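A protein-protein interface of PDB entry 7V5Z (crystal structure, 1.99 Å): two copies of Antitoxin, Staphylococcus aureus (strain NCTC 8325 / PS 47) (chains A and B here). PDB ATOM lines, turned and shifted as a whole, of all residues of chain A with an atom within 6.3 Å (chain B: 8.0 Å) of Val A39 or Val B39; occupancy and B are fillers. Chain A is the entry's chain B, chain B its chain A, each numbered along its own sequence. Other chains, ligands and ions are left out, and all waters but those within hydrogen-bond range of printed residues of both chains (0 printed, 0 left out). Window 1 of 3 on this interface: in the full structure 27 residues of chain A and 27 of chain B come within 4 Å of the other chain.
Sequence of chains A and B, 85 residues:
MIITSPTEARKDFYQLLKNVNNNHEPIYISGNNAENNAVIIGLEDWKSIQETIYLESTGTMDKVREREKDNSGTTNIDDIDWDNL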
ATOM      1  N   LEU A  17      18.347  -2.262  20.519  1.00  0.00           N
ATOM      2  CA  LEU A  17      18.521  -2.640  19.119  1.00  0.00           C
ATOM      3  C   LEU A  17      18.326  -4.142  18.914  1.00  0.00           C
ATOM      4  O   LEU A  17      17.808  -4.568  17.872  1.00  0.00           O
ATOM      5  CB  LEU A  17      19.904  -2.225  18.629  1.00  0.00           C
ATOM      6  CG  LEU A  17      20.233  -0.728  18.641  1.00  0.00           C
ATOM      7  CD1 LEU A  17      21.710  -0.506  18.334  1.00  0.00           C
ATOM      8  CD2 LEU A  17      19.372   0.012  17.646  1.00  0.00           C
ATOM      9  N   PRO A  26       8.286  -2.227  17.107  1.00  0.00           N
ATOM     10  CA  PRO A  26       8.987  -0.954  17.293  1.00  0.00           C
ATOM     11  C   PRO A  26       9.045  -0.592  18.764  1.00  0.00           C
ATOM     12  O   PRO A  26       8.273  -1.088  19.590  1.00  0.00           O
ATOM     13  CB  PRO A  26       8.130   0.043  16.507  1.00  0.00           C
ATOM     14  CG  PRO A  26       6.754  -0.578  16.482  1.00  0.00           C
ATOM     15  CD  PRO A  26       6.990  -2.063  16.425  1.00  0.00           C
ATOM     16  N   ILE A  27       9.983   0.290  19.097  1.00  0.00           N
ATOM     17  CA  ILE A  27      10.095   0.829  20.447  1.00  0.00           C
ATOM     18  C   ILE A  27       9.890   2.329  20.367  1.00  0.00           C
ATOM     19  O   ILE A  27      10.521   3.005  19.547  1.00  0.00           O
ATOM     20  CB  ILE A  27      11.442   0.470  21.100  1.00  0.00           C
ATOM     21  CG1 ILE A  27      11.469  -1.035  21.408  1.00  0.00           C
ATOM     22  CG2 ILE A  27      11.640   1.269  22.384  1.00  0.00           C
ATOM     23  CD1 ILE A  27      12.833  -1.581  21.863  1.00  0.00           C
ATOM     24  N   TYR A  28       9.001   2.845  21.205  1.00  0.00           N
ATOM     25  CA  TYR A  28       8.669   4.259  21.192  1.00  0.00           C
ATOM     26  C   TYR A  28       9.526   4.995  22.209  1.00  0.00           C
ATOM     27  O   TYR A  28       9.607   4.584  23.369  1.00  0.00           O
ATOM     28  CB  TYR A  28       7.185   4.465  21.501  1.00  0.00           C
ATOM     29  CG  TYR A  28       6.296   3.956  20.395  1.00  0.00           C
ATOM     30  CD1 TYR A  28       5.928   2.616  20.335  1.00  0.00           C
ATOM     31  CD2 TYR A  28       5.860   4.804  19.385  1.00  0.00           C
ATOM     32  CE1 TYR A  28       5.119   2.143  19.311  1.00  0.00           C
ATOM     33  CE2 TYR A  28       5.056   4.350  18.366  1.00  0.00           C
ATOM     34  CZ  TYR A  28       4.682   3.016  18.330  1.00  0.00           C
ATOM     35  OH  TYR A  28       3.879   2.559  17.304  1.00  0.00           O
ATOM     36  N   ILE A  29      10.174   6.070  21.765  1.00  0.00           N
ATOM     37  CA  ILE A  29      10.965   6.937  22.627  1.00  0.00           C
ATOM     38  C   ILE A  29      10.135   8.186  22.871  1.00  0.00           C
ATOM     39  O   ILE A  29       9.888   8.965  21.944  1.00  0.00           O
ATOM     40  CB  ILE A  29      12.321   7.285  22.005  1.00  0.00           C
ATOM     41  CG1 ILE A  29      13.086   6.009  21.658  1.00  0.00           C
ATOM     42  CG2 ILE A  29      13.129   8.161  22.953  1.00  0.00           C
ATOM     43  CD1 ILE A  29      14.269   6.259  20.751  1.00  0.00           C
ATOM     44  N   ASN A  37      10.046  13.202  20.068  1.00  0.00           N
ATOM     45  CA  ASN A  37       9.667  11.805  20.195  1.00  0.00           C
ATOM     46  C   ASN A  37      10.065  11.045  18.936  1.00  0.00           C
ATOM     47  O   ASN A  37      10.100  11.602  17.836  1.00  0.00           O
ATOM     48  CB  ASN A  37       8.167  11.688  20.452  1.00  0.00           C
ATOM     49  CG  ASN A  37       7.801  12.009  21.896  1.00  0.00           C
ATOM     50  OD1 ASN A  37       8.672  12.279  22.717  1.00  0.00           O
ATOM     51  ND2 ASN A  37       6.516  11.967  22.209  1.00  0.00           N
ATOM     52  N   ALA A  38      10.400   9.767  19.111  1.00  0.00           N
ATOM     53  CA  ALA A  38      10.947   8.973  18.017  1.00  0.00           C
ATOM     54  C   ALA A  38      10.549   7.519  18.195  1.00  0.00           C
ATOM     55  O   ALA A  38       9.980   7.117  19.219  1.00  0.00           O
ATOM     56  CB  ALA A  38      12.471   9.093  17.929  1.00  0.00           C
ATOM     57  N   VAL A  39      10.838   6.738  17.161  1.00  0.00           N
ATOM     58  CA  VAL A  39      10.557   5.310  17.127  1.00  0.00           C
ATOM     59  C   VAL A  39      11.801   4.600  16.612  1.00  0.00           C
ATOM     60  O   VAL A  39      12.431   5.060  15.653  1.00  0.00           O
ATOM     61  CB  VAL A  39       9.337   4.991  16.230  1.00  0.00           C
ATOM     62  CG1 VAL A  39       9.062   3.483  16.195  1.00  0.00           C
ATOM     63  CG2 VAL A  39       8.095   5.733  16.714  1.00  0.00           C
ATOM     64  N   ILE A  40      12.159   3.484  17.248  1.00  0.00           N
ATOM     65  CA  ILE A  40      13.204   2.596  16.751  1.00  0.00           C
ATOM     66  C   ILE A  40      12.535   1.377  16.139  1.00  0.00           C
ATOM     67  O   ILE A  40      11.682   0.750  16.775  1.00  0.00           O
ATOM     68  CB  ILE A  40      14.166   2.168  17.871  1.00  0.00           C
ATOM     69  CG1 ILE A  40      14.627   3.365  18.696  1.00  0.00           C
ATOM     70  CG2 ILE A  40      15.383   1.454  17.286  1.00  0.00           C
ATOM     71  CD1 ILE A  40      15.191   2.926  20.036  1.00  0.00           C
ATOM     72  N   ILE A  41      12.921   1.026  14.921  1.00  0.00           N
ATOM     73  CA  ILE A  41      12.359  -0.131  14.242  1.00  0.00           C
ATOM     74  C   ILE A  41      13.501  -0.953  13.662  1.00  0.00           C
ATOM     75  O   ILE A  41      14.467  -0.398  13.129  1.00  0.00           O
ATOM     76  CB  ILE A  41      11.351   0.292  13.145  1.00  0.00           C
ATOM     77  CG1 ILE A  41      10.780  -0.942  12.445  1.00  0.00           C
ATOM     78  CG2 ILE A  41      11.971   1.231  12.139  1.00  0.00           C
ATOM     79  CD1 ILE A  41       9.295  -0.829  12.122  1.00  0.00           C
ATOM     80  N   GLY A  42      13.406  -2.279  13.795  1.00  0.00           N
ATOM     81  CA  GLY A  42      14.384  -3.145  13.162  1.00  0.00           C
ATOM     82  C   GLY A  42      14.442  -2.913  11.659  1.00  0.00           C
ATOM     83  O   GLY A  42      13.451  -2.564  11.026  1.00  0.00           O
ATOM     84  N   LEU A  43      15.628  -3.106  11.086  1.00  0.00           N
ATOM     85  CA  LEU A  43      15.811  -2.753   9.680  1.00  0.00           C
ATOM     86  C   LEU A  43      14.965  -3.639   8.772  1.00  0.00           C
ATOM     87  O   LEU A  43      14.405  -3.167   7.777  1.00  0.00           O
ATOM     88  CB  LEU A  43      17.294  -2.841   9.299  1.00  0.00           C
ATOM     89  CG  LEU A  43      17.591  -2.647   7.805  1.00  0.00           C
ATOM     90  CD1 LEU A  43      17.281  -1.207   7.373  1.00  0.00           C
ATOM     91  CD2 LEU A  43      19.031  -3.018   7.463  1.00  0.00           C
ATOM     92  N   TRP A  46      11.510  -2.256   8.753  1.00  0.00           N
ATOM     93  CA  TRP A  46      11.525  -1.004   8.001  1.00  0.00           C
ATOM     94  C   TRP A  46      11.559  -1.271   6.501  1.00  0.00           C
ATOM     95  O   TRP A  46      10.816  -0.650   5.730  1.00  0.00           O
ATOM     96  CB  TRP A  46      12.727  -0.157   8.424  1.00  0.00           C
ATOM     97  CG  TRP A  46      12.929   1.106   7.601  1.00  0.00           C
ATOM     98  CD1 TRP A  46      13.837   1.301   6.592  1.00  0.00           C
ATOM     99  CD2 TRP A  46      12.221   2.349   7.744  1.00  0.00           C
ATOM    100  NE1 TRP A  46      13.725   2.584   6.095  1.00  0.00           N
ATOM    101  CE2 TRP A  46      12.746   3.246   6.792  1.00  0.00           C
ATOM    102  CE3 TRP A  46      11.188   2.783   8.577  1.00  0.00           C
ATOM    103  CZ2 TRP A  46      12.270   4.549   6.653  1.00  0.00           C
ATOM    104  CZ3 TRP A  46      10.721   4.090   8.440  1.00  0.00           C
ATOM    105  CH2 TRP A  46      11.263   4.949   7.486  1.00  0.00           C
ATOM    106  N   MET B   1      20.789   9.347   2.507  1.00  0.00           N
ATOM    107  CA  MET B   1      20.876   8.336   3.561  1.00  0.00           C
ATOM    108  C   MET B   1      21.848   8.745   4.675  1.00  0.00           C
ATOM    109  O   MET B   1      23.034   8.982   4.428  1.00  0.00           O
ATOM    110  CB  MET B   1      21.304   6.983   2.975  1.00  0.00           C
ATOM    111  CG  MET B   1      20.172   5.981   2.757  1.00  0.00           C
ATOM    112  SD  MET B   1      20.754   4.265   2.772  1.00  0.00           S
ATOM    113  CE  MET B   1      19.201   3.364   2.772  1.00  0.00           C
ATOM    114  N   ILE B   2      21.335   8.834   5.899  1.00  0.00           N
ATOM    115  CA  ILE B   2      22.144   9.143   7.075  1.00  0.00           C
ATOM    116  C   ILE B   2      22.418   7.835   7.805  1.00  0.00           C
ATOM    117  O   ILE B   2      21.486   7.168   8.270  1.00  0.00           O
ATOM    118  CB  ILE B   2      21.443  10.159   7.989  1.00  0.00           C
ATOM    119  CG1 ILE B   2      20.791  11.260   7.144  1.00  0.00           C
ATOM    120  CG2 ILE B   2      22.423  10.734   9.007  1.00  0.00           C
ATOM    121  CD1 ILE B   2      20.335  12.466   7.942  1.00  0.00           C
ATOM    122  N   LEU B  17      17.963  12.416  17.985  1.00  0.00           N
ATOM    123  CA  LEU B  17      16.516  12.530  18.147  1.00  0.00           C
ATOM    124  C   LEU B  17      16.011  13.873  17.643  1.00  0.00           C
ATOM    125  O   LEU B  17      14.969  13.943  16.978  1.00  0.00           O
ATOM    126  CB  LEU B  17      16.122  12.331  19.613  1.00  0.00           C
ATOM    127  CG  LEU B  17      16.421  10.943  20.172  1.00  0.00           C
ATOM    128  CD1 LEU B  17      16.089  10.833  21.663  1.00  0.00           C
ATOM    129  CD2 LEU B  17      15.630   9.925  19.389  1.00  0.00           C
ATOM    130  N   VAL B  20      16.301  13.715  13.591  1.00  0.00           N
ATOM    131  CA  VAL B  20      15.309  12.973  12.822  1.00  0.00           C
ATOM    132  C   VAL B  20      13.990  13.713  12.782  1.00  0.00           C
ATOM    133  O   VAL B  20      13.217  13.535  11.838  1.00  0.00           O
ATOM    134  CB  VAL B  20      15.100  11.539  13.353  1.00  0.00           C
ATOM    135  CG1 VAL B  20      16.429  10.822  13.451  1.00  0.00           C
ATOM    136  CG2 VAL B  20      14.365  11.541  14.699  1.00  0.00           C
ATOM    137  N   ASN B  21      13.728  14.573  13.761  1.00  0.00           N
ATOM    138  CA  ASN B  21      12.472  15.310  13.798  1.00  0.00           C
ATOM    139  C   ASN B  21      12.522  16.634  13.042  1.00  0.00           C
ATOM    140  O   ASN B  21      11.484  17.096  12.554  1.00  0.00           O
ATOM    141  CB  ASN B  21      12.051  15.537  15.252  1.00  0.00           C
ATOM    142  CG  ASN B  21      11.360  14.330  15.831  1.00  0.00           C
ATOM    143  OD1 ASN B  21      10.278  13.954  15.382  1.00  0.00           O
ATOM    144  ND2 ASN B  21      11.991  13.691  16.802  1.00  0.00           N
ATOM    145  N   GLU B  25      14.016  12.892   8.298  1.00  0.00           N
ATOM    146  CA  GLU B  25      14.749  11.856   7.599  1.00  0.00           C
ATOM    147  C   GLU B  25      15.148  10.753   8.565  1.00  0.00           C
ATOM    148  O   GLU B  25      15.697  11.042   9.636  1.00  0.00           O
ATOM    149  CB  GLU B  25      16.002  12.425   6.917  1.00  0.00           C
ATOM    150  CG  GLU B  25      15.717  13.106   5.588  1.00  0.00           C
ATOM    151  CD  GLU B  25      14.729  12.332   4.728  1.00  0.00           C
ATOM    152  OE1 GLU B  25      15.089  11.234   4.246  1.00  0.00           O
ATOM    153  OE2 GLU B  25      13.596  12.825   4.530  1.00  0.00           O
ATOM    154  N   PRO B  26      14.915   9.492   8.226  1.00  0.00           N
ATOM    155  CA  PRO B  26      15.345   8.406   9.107  1.00  0.00           C
ATOM    156  C   PRO B  26      16.860   8.341   9.182  1.00  0.00           C
ATOM    157  O   PRO B  26      17.571   8.740   8.256  1.00  0.00           O
ATOM    158  CB  PRO B  26      14.776   7.159   8.426  1.00  0.00           C
ATOM    159  CG  PRO B  26      14.768   7.521   6.982  1.00  0.00           C
ATOM    160  CD  PRO B  26      14.418   8.987   6.935  1.00  0.00           C
ATOM    161  N   ILE B  27      17.358   7.823  10.300  1.00  0.00           N
ATOM    162  CA  ILE B  27      18.781   7.557  10.457  1.00  0.00           C
ATOM    163  C   ILE B  27      18.970   6.053  10.596  1.00  0.00           C
ATOM    164  O   ILE B  27      18.276   5.400  11.383  1.00  0.00           O
ATOM    165  CB  ILE B  27      19.379   8.318  11.652  1.00  0.00           C
ATOM    166  CG1 ILE B  27      20.864   7.977  11.822  1.00  0.00           C
ATOM    167  CG2 ILE B  27      18.603   8.025  12.901  1.00  0.00           C
ATOM    168  CD1 ILE B  27      21.716   9.174  12.211  1.00  0.00           C
ATOM    169  N   TYR B  28      19.875   5.504   9.801  1.00  0.00           N
ATOM    170  CA  TYR B  28      20.123   4.072   9.798  1.00  0.00           C
ATOM    171  C   TYR B  28      21.229   3.777  10.802  1.00  0.00           C
ATOM    172  O   TYR B  28      22.314   4.369  10.738  1.00  0.00           O
ATOM    173  CB  TYR B  28      20.485   3.587   8.396  1.00  0.00           C
ATOM    174  CG  TYR B  28      19.311   3.652   7.433  1.00  0.00           C
ATOM    175  CD1 TYR B  28      18.493   2.544   7.234  1.00  0.00           C
ATOM    176  CD2 TYR B  28      19.006   4.826   6.743  1.00  0.00           C
ATOM    177  CE1 TYR B  28      17.409   2.593   6.367  1.00  0.00           C
ATOM    178  CE2 TYR B  28      17.915   4.889   5.869  1.00  0.00           C
ATOM    179  CZ  TYR B  28      17.122   3.762   5.692  1.00  0.00           C
ATOM    180  OH  TYR B  28      16.044   3.786   4.837  1.00  0.00           O
ATOM    181  N   ILE B  29      20.922   2.913  11.759  1.00  0.00           N
ATOM    182  CA  ILE B  29      21.907   2.366  12.678  1.00  0.00           C
ATOM    183  C   ILE B  29      22.394   1.071  12.050  1.00  0.00           C
ATOM    184  O   ILE B  29      21.633   0.107  11.937  1.00  0.00           O
ATOM    185  CB  ILE B  29      21.311   2.110  14.065  1.00  0.00           C
ATOM    186  CG1 ILE B  29      20.454   3.294  14.544  1.00  0.00           C
ATOM    187  CG2 ILE B  29      22.401   1.719  15.050  1.00  0.00           C
ATOM    188  CD1 ILE B  29      21.174   4.615  14.621  1.00  0.00           C
ATOM    189  N   SER B  30      23.650   1.045  11.620  1.00  0.00           N
ATOM    190  CA  SER B  30      24.220  -0.135  10.982  1.00  0.00           C
ATOM    191  C   SER B  30      25.487  -0.527  11.729  1.00  0.00           C
ATOM    192  O   SER B  30      26.442   0.258  11.797  1.00  0.00           O
ATOM    193  CB  SER B  30      24.512   0.130   9.506  1.00  0.00           C
ATOM    194  OG  SER B  30      25.606  -0.655   9.069  1.00  0.00           O
ATOM    195  N   ASN B  36      21.066  -6.717  14.410  1.00  0.00           N
ATOM    196  CA  ASN B  36      20.630  -5.614  15.245  1.00  0.00           C
ATOM    197  C   ASN B  36      20.760  -4.254  14.561  1.00  0.00           C
ATOM    198  O   ASN B  36      20.781  -3.233  15.249  1.00  0.00           O
ATOM    199  CB  ASN B  36      21.414  -5.688  16.544  1.00  0.00           C
ATOM    200  CG  ASN B  36      21.350  -7.081  17.152  1.00  0.00           C
ATOM    201  OD1 ASN B  36      20.421  -7.843  16.884  1.00  0.00           O
ATOM    202  ND2 ASN B  36      22.378  -7.443  17.921  1.00  0.00           N
ATOM    203  N   ASN B  37      20.845  -4.224  13.230  1.00  0.00           N
ATOM    204  CA  ASN B  37      20.661  -2.982  12.486  1.00  0.00           C
ATOM    205  C   ASN B  37      19.240  -2.470  12.684  1.00  0.00           C
ATOM    206  O   ASN B  37      18.297  -3.257  12.764  1.00  0.00           O
ATOM    207  CB  ASN B  37      20.914  -3.210  10.997  1.00  0.00           C
ATOM    208  CG  ASN B  37      22.382  -3.477  10.685  1.00  0.00           C
ATOM    209  OD1 ASN B  37      23.238  -3.432  11.568  1.00  0.00           O
ATOM    210  ND2 ASN B  37      22.670  -3.768   9.430  1.00  0.00           N
ATOM    211  N   ALA B  38      19.086  -1.146  12.736  1.00  0.00           N
ATOM    212  CA  ALA B  38      17.798  -0.534  13.026  1.00  0.00           C
ATOM    213  C   ALA B  38      17.697   0.827  12.343  1.00  0.00           C
ATOM    214  O   ALA B  38      18.653   1.334  11.743  1.00  0.00           O
ATOM    215  CB  ALA B  38      17.573  -0.386  14.538  1.00  0.00           C
ATOM    216  N   VAL B  39      16.507   1.410  12.438  1.00  0.00           N
ATOM    217  CA  VAL B  39      16.209   2.729  11.892  1.00  0.00           C
ATOM    218  C   VAL B  39      15.522   3.531  12.984  1.00  0.00           C
ATOM    219  O   VAL B  39      14.653   3.009  13.692  1.00  0.00           O
ATOM    220  CB  VAL B  39      15.307   2.651  10.639  1.00  0.00           C
ATOM    221  CG1 VAL B  39      15.019   4.044  10.101  1.00  0.00           C
ATOM    222  CG2 VAL B  39      15.940   1.771   9.551  1.00  0.00           C
ATOM    223  N   ILE B  40      15.898   4.793  13.115  1.00  0.00           N
ATOM    224  CA  ILE B  40      15.241   5.719  14.028  1.00  0.00           C
ATOM    225  C   ILE B  40      14.520   6.746  13.180  1.00  0.00           C
ATOM    226  O   ILE B  40      15.096   7.275  12.225  1.00  0.00           O
ATOM    227  CB  ILE B  40      16.244   6.377  14.987  1.00  0.00           C
ATOM    228  CG1 ILE B  40      16.814   5.297  15.915  1.00  0.00           C
ATOM    229  CG2 ILE B  40      15.566   7.438  15.790  1.00  0.00           C
ATOM    230  CD1 ILE B  40      17.913   5.786  16.847  1.00  0.00           C
ATOM    231  N   ILE B  41      13.253   6.999  13.507  1.00  0.00           N
ATOM    232  CA  ILE B  41      12.398   7.889  12.730  1.00  0.00           C
ATOM    233  C   ILE B  41      11.615   8.765  13.707  1.00  0.00           C
ATOM    234  O   ILE B  41      11.267   8.336  14.815  1.00  0.00           O
ATOM    235  CB  ILE B  41      11.456   7.063  11.803  1.00  0.00           C
ATOM    236  CG1 ILE B  41      10.579   7.954  10.911  1.00  0.00           C
ATOM    237  CG2 ILE B  41      10.589   6.122  12.624  1.00  0.00           C
ATOM    238  CD1 ILE B  41      11.361   8.593   9.741  1.00  0.00           C
ATOM    239  N   GLY B  42      11.352  10.005  13.300  1.00  0.00           N
ATOM    240  CA  GLY B  42      10.529  10.878  14.117  1.00  0.00           C
ATOM    241  C   GLY B  42       9.137  10.307  14.314  1.00  0.00           C
ATOM    242  O   GLY B  42       8.593   9.620  13.447  1.00  0.00           O
ATOM    243  N   LEU B  43       8.560  10.578  15.490  1.00  0.00           N
ATOM    244  CA  LEU B  43       7.254  10.006  15.813  1.00  0.00           C
ATOM    245  C   LEU B  43       6.199  10.445  14.808  1.00  0.00           C
ATOM    246  O   LEU B  43       5.359   9.646  14.380  1.00  0.00           O
ATOM    247  CB  LEU B  43       6.843  10.411  17.225  1.00  0.00           C
ATOM    248  CG  LEU B  43       5.424   9.982  17.595  1.00  0.00           C
ATOM    249  CD1 LEU B  43       5.302   8.464  17.569  1.00  0.00           C
ATOM    250  CD2 LEU B  43       5.000  10.562  18.943  1.00  0.00           C
ATOM    251  N   GLU B  44       6.227  11.718  14.424  1.00  0.00           N
ATOM    252  CA  GLU B  44       5.259  12.230  13.463  1.00  0.00           C
ATOM    253  C   GLU B  44       5.371  11.494  12.134  1.00  0.00           C
ATOM    254  O   GLU B  44       4.360  11.069  11.561  1.00  0.00           O
ATOM    255  CB  GLU B  44       5.478  13.731  13.278  1.00  0.00           C
ATOM    256  CG  GLU B  44       4.281  14.491  12.822  1.00  0.00           C
ATOM    257  CD  GLU B  44       4.376  15.951  13.215  1.00  0.00           C
ATOM    258  OE1 GLU B  44       3.810  16.326  14.271  1.00  0.00           O
ATOM    259  OE2 GLU B  44       5.043  16.714  12.478  1.00  0.00           O
ATOM    260  N   ASP B  45       6.600  11.321  11.632  1.00  0.00           N
ATOM    261  CA  ASP B  45       6.788  10.563  10.397  1.00  0.00           C
ATOM    262  C   ASP B  45       6.353   9.113  10.564  1.00  0.00           C
ATOM    263  O   ASP B  45       5.845   8.497   9.618  1.00  0.00           O
ATOM    264  CB  ASP B  45       8.247  10.630   9.947  1.00  0.00           C
ATOM    265  CG  ASP B  45       8.663  12.029   9.558  1.00  0.00           C
ATOM    266  OD1 ASP B  45       7.769  12.883   9.385  1.00  0.00           O
ATOM    267  OD2 ASP B  45       9.878  12.278   9.418  1.00  0.00           O
ATOM    268  N   TRP B  46       6.566   8.536  11.750  1.00  0.00           N
ATOM    269  CA  TRP B  46       6.120   7.158  11.969  1.00  0.00           C
ATOM    270  C   TRP B  46       4.596   7.066  11.930  1.00  0.00           C
ATOM    271  O   TRP B  46       4.033   6.121  11.357  1.00  0.00           O
ATOM    272  CB  TRP B  46       6.665   6.629  13.296  1.00  0.00           C
ATOM    273  CG  TRP B  46       6.157   5.263  13.676  1.00  0.00           C
ATOM    274  CD1 TRP B  46       5.320   4.957  14.714  1.00  0.00           C
ATOM    275  CD2 TRP B  46       6.462   4.019  13.031  1.00  0.00           C
ATOM    276  NE1 TRP B  46       5.081   3.603  14.746  1.00  0.00           N
ATOM    277  CE2 TRP B  46       5.767   3.006  13.723  1.00  0.00           C
ATOM    278  CE3 TRP B  46       7.240   3.666  11.923  1.00  0.00           C
ATOM    279  CZ2 TRP B  46       5.834   1.667  13.353  1.00  0.00           C
ATOM    280  CZ3 TRP B  46       7.306   2.321  11.554  1.00  0.00           C
ATOM    281  CH2 TRP B  46       6.606   1.344  12.272  1.00  0.00           C
ATOM    282  N   LYS B  47       3.909   8.049  12.516  1.00  0.00           N
ATOM    283  CA  LYS B  47       2.450   8.014  12.515  1.00  0.00           C
ATOM    284  C   LYS B  47       1.892   8.134  11.098  1.00  0.00           C
ATOM    285  O   LYS B  47       0.875   7.503  10.774  1.00  0.00           O
ATOM    286  CB  LYS B  47       1.905   9.118  13.414  1.00  0.00           C
ATOM    287  CG  LYS B  47       2.033   8.799  14.892  1.00  0.00           C
ATOM    288  CD  LYS B  47       1.677  10.022  15.738  1.00  0.00           C
ATOM    289  CE  LYS B  47       0.165  10.295  15.775  1.00  0.00           C
ATOM    290  NZ  LYS B  47      -0.171  11.658  16.332  1.00  0.00           N
ATOM    291  N   GLN B  50       2.459   4.616   9.740  1.00  0.00           N
ATOM    292  CA  GLN B  50       1.468   3.725  10.337  1.00  0.00           C
ATOM    293  C   GLN B  50       0.097   3.920   9.706  1.00  0.00           C
ATOM    294  O   GLN B  50      -0.626   2.951   9.441  1.00  0.00           O
ATOM    295  CB  GLN B  50       1.362   3.990  11.837  1.00  0.00           C
ATOM    296  CG  GLN B  50       2.243   3.135  12.730  1.00  0.00           C
ATOM    297  CD  GLN B  50       1.964   3.421  14.201  1.00  0.00           C
ATOM    298  OE1 GLN B  50       1.546   4.531  14.557  1.00  0.00           O
ATOM    299  NE2 GLN B  50       2.191   2.427  15.059  1.00  0.00           N
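N of Leu A43 is in hydrogen-bond range of O of Asn B37, at 3.2 Å. N of Leu B43 sits at hydrogen-bond distance from O of Asn A37 (3.0 Å). OH of Tyr A28 sits at hydrogen-bond distance from NE2 of Gln B50 (2.8 Å). O of Ile B41 sits at hydrogen-bond distance from N of Val A39, 2.9 Å away. The backbone NH (N) of Val B39 lies within hydrogen-bond range of the backbone carbonyl oxygen (O) of Ile A41 (2.8 Å). The indole nitrogen (NE1) of Trp B46 lies within hydrogen-bond range of the side-chain hydroxyl (OH) of Tyr A28, 3.0 Å away. OH of Tyr B28 is in hydrogen-bond range of NE1 of Trp A46, at 2.9 Å. ND2 of Asn B21 sits at hydrogen-bond distance from O of Asn A37, 3.0 Å away.
Leu A17 touches Ala B38, and with the chains exchanged Ala A38 touches Leu B17. Tyr A28 touches Trp B46, and with the chains exchanged Trp A46 touches Tyr B28. Positions printed for both chains: 17, 26, 27, 28, 29, 37, 38, 39, 40, 41, 42, 43 and 46. Of the 29 pairs that touch across the chains among the printed residues, 23 have their exchanged pair printed and touching as well.
Of the 13 printed residues of chain A, 11 touch a printed residue of chain B. Hydrophobic or aromatic side chains of chain A within 4 Å of the printed part of chain B: Leu A17, Pro A26, Tyr A28, Ala A38, Val A39, Ile A40, Ile A41, Leu A43 and Trp A46. Along chain A the printed residues that touch a printed residue of chain B span positions 17 to 46. Hydrophobic or aromatic side chains of chain B within 4 Å of the printed part of chain A: Leu B17, Pro B26, Tyr B28, Ala B38, Val B39, Ile B40, Ile B41, Leu B43 and Trp B46. Along chain B the printed residues that touch a printed residue of chain A span positions 17 to 50. Among the printed residues, no Asp or Glu carboxylate lies within 4 Å of a Lys or Arg side-chain nitrogen of the other chain.
Among the printed residues, pairs that only touch across the chains: Ala A38 with Ile B41, Val A39 with Ile B40, Ile A41 with Ala B38, Ile A40 with Val B39, Ile A41 with Trp B46, Val A39 with Trp B46, Ala A38 with Leu B17, Val A39 with Val B39, Leu A17 with Ala B38, Leu A17 with Asn B36, Trp A46 with Val B39, Asn A37 with Gly B42, Ala A38 with Leu B43, Leu A43 with Ala B38, Trp A46 with Pro B26, Leu A43 with Val B39, Leu A43 with Tyr B28, Gly A42 with Asn B37, Pro A26 with Trp B46, Ile A40 with Ala B38 and Val A39 with Leu B43.
O of Ile A27 is in hydrogen-bond range of N of Ile A40, 2.9 Å away. O of Ile B27 sits at hydrogen-bond distance from N of Ile B40 (3.0 Å). O of Ile B2 is in hydrogen-bond range of N of Tyr B28, 2.8 Å away. The backbone carbonyl oxygen of Ala B38 lies within hydrogen-bond range of the backbone NH of Ile B29. The side-chain amide nitrogen (NE2) of Gln B50 sits close to the indole nitrogen (NE1) of Trp B46 (3.1 Å).
Ala A38 touches three residues of chain B. Printed residues of chain B within 4 Å of Val A39: Val B39, Ile B40, Ile B41, Leu B43 and Trp B46. Of the printed residues of chain B, Ile A40 touches Ala B38 (3.97 Å) and Val B39 (3.4 Å). Ser B30 touches none of the printed residues of chain A. Printed residues of chain A within 4 Å of Asn B36: Leu A17 (3.6 Å). Printed residues of chain A within 4 Å of Ala B38: Leu A17, Ile A40, Ile A41 and Leu A43. Val B39 touches just these residues of chain A: Val A39, Ile A40, Ile A41, Leu A43 and Trp A46. Of the printed residues of chain A, Gln B50 touches Tyr A28 (2.8 Å). The nearest residue of chain A that does not touch Val B39 is Gly A42 (4.9 Å). The nearest printed residue of chain A that does not touch Asn B21 is Ala A38 (4.8 Å).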
